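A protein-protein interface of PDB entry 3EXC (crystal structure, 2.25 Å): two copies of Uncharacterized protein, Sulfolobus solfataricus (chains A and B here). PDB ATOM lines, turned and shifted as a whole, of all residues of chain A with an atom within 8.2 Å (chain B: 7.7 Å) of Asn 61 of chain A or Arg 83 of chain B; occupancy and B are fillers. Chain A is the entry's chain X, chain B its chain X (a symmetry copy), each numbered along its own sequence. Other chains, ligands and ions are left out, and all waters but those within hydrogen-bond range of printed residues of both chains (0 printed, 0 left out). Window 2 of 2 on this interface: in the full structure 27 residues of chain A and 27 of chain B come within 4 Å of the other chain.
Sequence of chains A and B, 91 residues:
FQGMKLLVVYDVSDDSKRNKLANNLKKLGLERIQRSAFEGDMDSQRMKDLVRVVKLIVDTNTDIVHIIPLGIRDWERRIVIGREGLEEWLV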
ATOM      1  N   ASP A  11      30.535  16.271   4.398  1.00  0.00           N
ATOM      2  CA  ASP A  11      29.151  16.299   3.995  1.00  0.00           C
ATOM      3  C   ASP A  11      28.447  16.579   5.341  1.00  0.00           C
ATOM      4  O   ASP A  11      28.137  15.682   6.151  1.00  0.00           O
ATOM      5  CB  ASP A  11      28.842  14.936   3.333  1.00  0.00           C
ATOM      6  CG  ASP A  11      27.341  14.671   3.123  1.00  0.00           C
ATOM      7  OD1 ASP A  11      26.495  15.525   3.546  1.00  0.00           O
ATOM      8  OD2 ASP A  11      27.002  13.560   2.559  1.00  0.00           O
ATOM      9  N   VAL A  12      28.277  17.863   5.618  1.00  0.00           N
ATOM     10  CA  VAL A  12      27.741  18.283   6.855  1.00  0.00           C
ATOM     11  C   VAL A  12      26.386  18.938   6.603  1.00  0.00           C
ATOM     12  O   VAL A  12      26.350  20.002   5.998  1.00  0.00           O
ATOM     13  CB  VAL A  12      28.677  19.288   7.534  1.00  0.00           C
ATOM     14  CG1 VAL A  12      27.985  19.914   8.705  1.00  0.00           C
ATOM     15  CG2 VAL A  12      29.975  18.568   7.982  1.00  0.00           C
ATOM     16  N   SER A  13      25.287  18.305   7.047  1.00  0.00           N
ATOM     17  CA  SER A  13      23.924  18.857   6.829  1.00  0.00           C
ATOM     18  C   SER A  13      23.639  20.234   7.432  1.00  0.00           C
ATOM     19  O   SER A  13      23.277  21.133   6.688  1.00  0.00           O
ATOM     20  CB  SER A  13      22.813  17.859   7.187  1.00  0.00           C
ATOM     21  OG  SER A  13      22.649  16.970   6.079  1.00  0.00           O
ATOM     22  N   VAL A  58      30.924  17.939  14.027  1.00  0.00           N
ATOM     23  CA  VAL A  58      29.895  17.432  13.152  1.00  0.00           C
ATOM     24  C   VAL A  58      28.933  16.554  13.956  1.00  0.00           C
ATOM     25  O   VAL A  58      29.309  16.050  15.039  1.00  0.00           O
ATOM     26  CB  VAL A  58      30.498  16.619  11.977  1.00  0.00           C
ATOM     27  CG1 VAL A  58      31.534  17.509  11.217  1.00  0.00           C
ATOM     28  CG2 VAL A  58      31.071  15.276  12.469  1.00  0.00           C
ATOM     29  N   ASP A  59      27.714  16.366  13.419  1.00  0.00           N
ATOM     30  CA  ASP A  59      26.754  15.360  13.932  1.00  0.00           C
ATOM     31  C   ASP A  59      27.153  14.020  13.367  1.00  0.00           C
ATOM     32  O   ASP A  59      26.955  13.742  12.226  1.00  0.00           O
ATOM     33  CB  ASP A  59      25.334  15.711  13.493  1.00  0.00           C
ATOM     34  CG  ASP A  59      24.273  14.696  13.964  1.00  0.00           C
ATOM     35  OD1 ASP A  59      24.541  13.460  14.187  1.00  0.00           O
ATOM     36  OD2 ASP A  59      23.118  15.172  14.058  1.00  0.00           O
ATOM     37  N   THR A  60      27.703  13.182  14.207  1.00  0.00           N
ATOM     38  CA  THR A  60      28.148  11.841  13.844  1.00  0.00           C
ATOM     39  C   THR A  60      27.094  10.789  13.431  1.00  0.00           C
ATOM     40  O   THR A  60      27.438   9.724  12.869  1.00  0.00           O
ATOM     41  CB  THR A  60      28.953  11.383  15.008  1.00  0.00           C
ATOM     42  OG1 THR A  60      30.246  11.960  14.817  1.00  0.00           O
ATOM     43  CG2 THR A  60      29.018   9.829  15.177  1.00  0.00           C
ATOM     44  N   ASN A  61      25.813  11.085  13.647  1.00  0.00           N
ATOM     45  CA  ASN A  61      24.798  10.161  13.173  1.00  0.00           C
ATOM     46  C   ASN A  61      24.348  10.474  11.797  1.00  0.00           C
ATOM     47  O   ASN A  61      23.708   9.641  11.197  1.00  0.00           O
ATOM     48  CB  ASN A  61      23.595  10.181  14.089  1.00  0.00           C
ATOM     49  CG  ASN A  61      23.987   9.895  15.497  1.00  0.00           C
ATOM     50  OD1 ASN A  61      23.951  10.798  16.346  1.00  0.00           O
ATOM     51  ND2 ASN A  61      24.485   8.660  15.747  1.00  0.00           N
ATOM     52  N   THR A  62      24.700  11.667  11.322  1.00  0.00           N
ATOM     53  CA  THR A  62      24.109  12.364  10.172  1.00  0.00           C
ATOM     54  C   THR A  62      25.149  12.755   9.161  1.00  0.00           C
ATOM     55  O   THR A  62      24.854  12.751   7.985  1.00  0.00           O
ATOM     56  CB  THR A  62      23.513  13.730  10.652  1.00  0.00           C
ATOM     57  OG1 THR A  62      22.369  13.464  11.448  1.00  0.00           O
ATOM     58  CG2 THR A  62      23.187  14.769   9.504  1.00  0.00           C
ATOM     59  N   ASP A  63      26.303  13.229   9.643  1.00  0.00           N
ATOM     60  CA  ASP A  63      27.330  13.802   8.780  1.00  0.00           C
ATOM     61  C   ASP A  63      28.351  12.754   8.436  1.00  0.00           C
ATOM     62  O   ASP A  63      28.328  11.669   9.084  1.00  0.00           O
ATOM     63  CB  ASP A  63      27.933  15.044   9.403  1.00  0.00           C
ATOM     64  CG  ASP A  63      26.889  16.101   9.601  1.00  0.00           C
ATOM     65  OD1 ASP A  63      25.845  16.011   8.859  1.00  0.00           O
ATOM     66  OD2 ASP A  63      27.057  16.989  10.490  1.00  0.00           O
ATOM     67  N   ILE A  64      29.166  13.046   7.409  1.00  0.00           N
ATOM     68  CA  ILE A  64      30.241  12.161   6.953  1.00  0.00           C
ATOM     69  C   ILE A  64      31.427  13.042   6.676  1.00  0.00           C
ATOM     70  O   ILE A  64      31.283  14.061   6.024  1.00  0.00           O
ATOM     71  CB  ILE A  64      29.951  11.413   5.635  1.00  0.00           C
ATOM     72  CG1 ILE A  64      28.638  10.660   5.697  1.00  0.00           C
ATOM     73  CG2 ILE A  64      30.988  10.326   5.412  1.00  0.00           C
ATOM     74  CD1 ILE A  64      27.955  10.504   4.306  1.00  0.00           C
ATOM     75  N   VAL A  65      32.609  12.642   7.150  1.00  0.00           N
ATOM     76  CA  VAL A  65      33.852  13.314   6.898  1.00  0.00           C
ATOM     77  C   VAL A  65      34.882  12.254   6.558  1.00  0.00           C
ATOM     78  O   VAL A  65      35.010  11.238   7.258  1.00  0.00           O
ATOM     79  CB  VAL A  65      34.328  14.109   8.121  1.00  0.00           C
ATOM     80  CG1 VAL A  65      35.637  14.864   7.762  1.00  0.00           C
ATOM     81  CG2 VAL A  65      33.302  15.215   8.511  1.00  0.00           C
ATOM     82  N   HIS A  66      35.619  12.462   5.478  1.00  0.00           N
ATOM     83  CA  HIS A  66      36.687  11.575   5.131  1.00  0.00           C
ATOM     84  C   HIS A  66      38.005  12.275   5.334  1.00  0.00           C
ATOM     85  O   HIS A  66      38.178  13.421   4.929  1.00  0.00           O
ATOM     86  CB  HIS A  66      36.588  11.309   3.682  1.00  0.00           C
ATOM     87  CG  HIS A  66      35.682  10.197   3.379  1.00  0.00           C
ATOM     88  ND1 HIS A  66      34.312  10.335   3.449  1.00  0.00           N
ATOM     89  CD2 HIS A  66      35.928   8.896   3.068  1.00  0.00           C
ATOM     90  CE1 HIS A  66      33.746   9.155   3.220  1.00  0.00           C
ATOM     91  NE2 HIS A  66      34.701   8.268   2.975  1.00  0.00           N
ATOM     92  N   ILE B  33      30.822   7.933  -2.024  1.00  0.00           N
ATOM     93  CA  ILE B  33      31.238   7.837  -0.622  1.00  0.00           C
ATOM     94  C   ILE B  33      30.650   8.986   0.213  1.00  0.00           C
ATOM     95  O   ILE B  33      30.616   8.862   1.419  1.00  0.00           O
ATOM     96  CB  ILE B  33      32.774   7.858  -0.445  1.00  0.00           C
ATOM     97  CG1 ILE B  33      33.331   9.115  -1.026  1.00  0.00           C
ATOM     98  CG2 ILE B  33      33.386   6.688  -1.114  1.00  0.00           C
ATOM     99  CD1 ILE B  33      34.899   9.418  -0.703  1.00  0.00           C
ATOM    100  N   ARG B  35      28.086  12.985  -0.119  1.00  0.00           N
ATOM    101  CA  ARG B  35      27.244  13.793  -0.996  1.00  0.00           C
ATOM    102  C   ARG B  35      27.947  14.354  -2.262  1.00  0.00           C
ATOM    103  O   ARG B  35      27.329  14.512  -3.338  1.00  0.00           O
ATOM    104  CB  ARG B  35      26.593  14.926  -0.214  1.00  0.00           C
ATOM    105  CG  ARG B  35      26.352  16.138  -1.009  1.00  0.00           C
ATOM    106  CD  ARG B  35      25.845  17.273  -0.148  1.00  0.00           C
ATOM    107  NE  ARG B  35      25.979  18.485  -0.937  1.00  0.00           N
ATOM    108  CZ  ARG B  35      25.021  18.972  -1.706  1.00  0.00           C
ATOM    109  NH1 ARG B  35      23.848  18.364  -1.767  1.00  0.00           N
ATOM    110  NH2 ARG B  35      25.235  20.066  -2.414  1.00  0.00           N
ATOM    111  N   VAL B  80      37.144   7.546   8.418  1.00  0.00           N
ATOM    112  CA  VAL B  80      35.856   8.055   8.088  1.00  0.00           C
ATOM    113  C   VAL B  80      35.086   8.334   9.376  1.00  0.00           C
ATOM    114  O   VAL B  80      34.914   7.475  10.259  1.00  0.00           O
ATOM    115  CB  VAL B  80      35.080   6.998   7.318  1.00  0.00           C
ATOM    116  CG1 VAL B  80      33.790   7.592   6.704  1.00  0.00           C
ATOM    117  CG2 VAL B  80      35.987   6.379   6.223  1.00  0.00           C
ATOM    118  N   ILE B  81      34.609   9.537   9.512  1.00  0.00           N
ATOM    119  CA  ILE B  81      33.804   9.894  10.658  1.00  0.00           C
ATOM    120  C   ILE B  81      32.373   9.963  10.213  1.00  0.00           C
ATOM    121  O   ILE B  81      32.090  10.522   9.174  1.00  0.00           O
ATOM    122  CB  ILE B  81      34.331  11.229  11.231  1.00  0.00           C
ATOM    123  CG1 ILE B  81      35.659  10.904  11.919  1.00  0.00           C
ATOM    124  CG2 ILE B  81      33.367  11.901  12.203  1.00  0.00           C
ATOM    125  CD1 ILE B  81      36.569  11.980  11.781  1.00  0.00           C
ATOM    126  N   GLY B  82      31.480   9.380  11.007  1.00  0.00           N
ATOM    127  CA  GLY B  82      30.040   9.524  10.864  1.00  0.00           C
ATOM    128  C   GLY B  82      29.368   8.414  10.070  1.00  0.00           C
ATOM    129  O   GLY B  82      30.014   7.407   9.698  1.00  0.00           O
ATOM    130  N   ARG B  83      28.095   8.665   9.730  1.00  0.00           N
ATOM    131  CA  ARG B  83      27.155   7.659   9.196  1.00  0.00           C
ATOM    132  C   ARG B  83      27.670   6.764   8.031  1.00  0.00           C
ATOM    133  O   ARG B  83      28.702   7.053   7.403  1.00  0.00           O
ATOM    134  CB  ARG B  83      25.836   8.365   8.814  1.00  0.00           C
ATOM    135  CG  ARG B  83      24.474   7.524   9.028  1.00  0.00           C
ATOM    136  CD  ARG B  83      23.347   7.892   7.954  1.00  0.00           C
ATOM    137  NE  ARG B  83      23.476   9.241   7.338  1.00  0.00           N
ATOM    138  CZ  ARG B  83      24.591   9.767   6.762  1.00  0.00           C
ATOM    139  NH1 ARG B  83      25.754   9.103   6.697  1.00  0.00           N
ATOM    140  NH2 ARG B  83      24.556  10.997   6.227  1.00  0.00           N
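The backbone carbonyl oxygen (O) of Thr 62 of chain A lies within hydrogen-bond range of the guanidinium group (NH2) of Arg 83 of chain B, 2.5 Å away. The backbone carbonyl oxygen (O) of Asp 63 of chain A sits at hydrogen-bond distance from the backbone NH (N) of Arg 83 of chain B. The side-chain carboxylate of Asp 11 of chain A sits at hydrogen-bond distance from the backbone NH of Arg 35 of chain B (2.9 Å). The backbone carbonyl oxygen (O) of Thr 60 of chain A is in hydrogen-bond range of the backbone NH (N) of Arg 83 of chain B, 3.4 Å away. The backbone carbonyl oxygen (O) of Val 65 of chain A is in hydrogen-bond range of the backbone NH (N) of Ile 81 of chain B, 2.9 Å away.
The side-chain carboxylate (OD1) of Asp 59 of chain A is in hydrogen-bond range of the backbone NH (N) of Asn 61 of chain A, at 2.7 Å. The backbone NH (N) of Asp 11 of chain A sits at hydrogen-bond distance from the backbone carbonyl oxygen (O) of Ile 64 of chain A, at 2.8 Å. OG1 of Thr 62 of chain A sits at hydrogen-bond distance from OD2 of Asp 59 of chain A, 3.2 Å away. The side-chain carboxylate of Asp 63 of chain A lies within hydrogen-bond range of the backbone NH of Ser 13 of chain A. The side-chain carboxylate (OD2) of Asp 63 of chain A lies within hydrogen-bond range of the backbone NH (N) of Asp 59 of chain A (3.1 Å).
Thr 60 of chain A touches Gly 82 of chain B (O to CA, 3.3 Å). Asn 61 of chain A touches Arg 83 of chain B (O to CG, 3.1 Å). O of Asp 63 of chain A touches O of Ile 81 of chain B, 3.9 Å away. O of Asp 63 of chain A touches CA of Gly 82 of chain B, 3.3 Å away. O of Ile 81 of chain B touches CA of Ile 64 of chain A, at 3.3 Å. Ile 64 of chain A touches Arg 83 of chain B. Val 65 of chain A touches Val 80 of chain B. Ile 33 of chain B touches His 66 of chain A. His 66 of chain A touches Val 80 of chain B.
Val 12 of chain A touches none of the printed residues of chain B. Asn 61 of chain A touches just one residue of chain B: Arg 83 (3.1 Å). Printed residues of chain B within 4 Å of Asp 63 of chain A: Ile 81 (3.9 Å), Gly 82 (3.3 Å) and Arg 83 (3.1 Å). Of the printed residues of chain B, Ile 64 of chain A touches Ile 81 and Arg 83. Of chain A, only Thr 60 and Asp 63 come within 4 Å of Gly 82 of chain B. Of the printed residues of chain A, Arg 83 of chain B touches Thr 60, Asn 61, Thr 62, Asp 63 and Ile 64. The nearest printed residue of chain A that does not touch Arg 35 of chain B is Ile 64 of chain A (5.1 Å).
Printed residues of chain B that touch a printed residue of chain A: Ile 33, Arg 35, Val 80, Ile 81, Gly 82 and Arg 83. Hydrophobic or aromatic side chains of chain B that line the printed part of chain A: Ile 33 and Val 80. Hydrophobic or aromatic side chains of chain A within 4 Å of the printed part of chain B: Ile 64 and His 66.
No position is printed for both chains. Of the 14 pairs that touch across the chains among the printed residues, none has its exchanged pair printed and touching as well.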
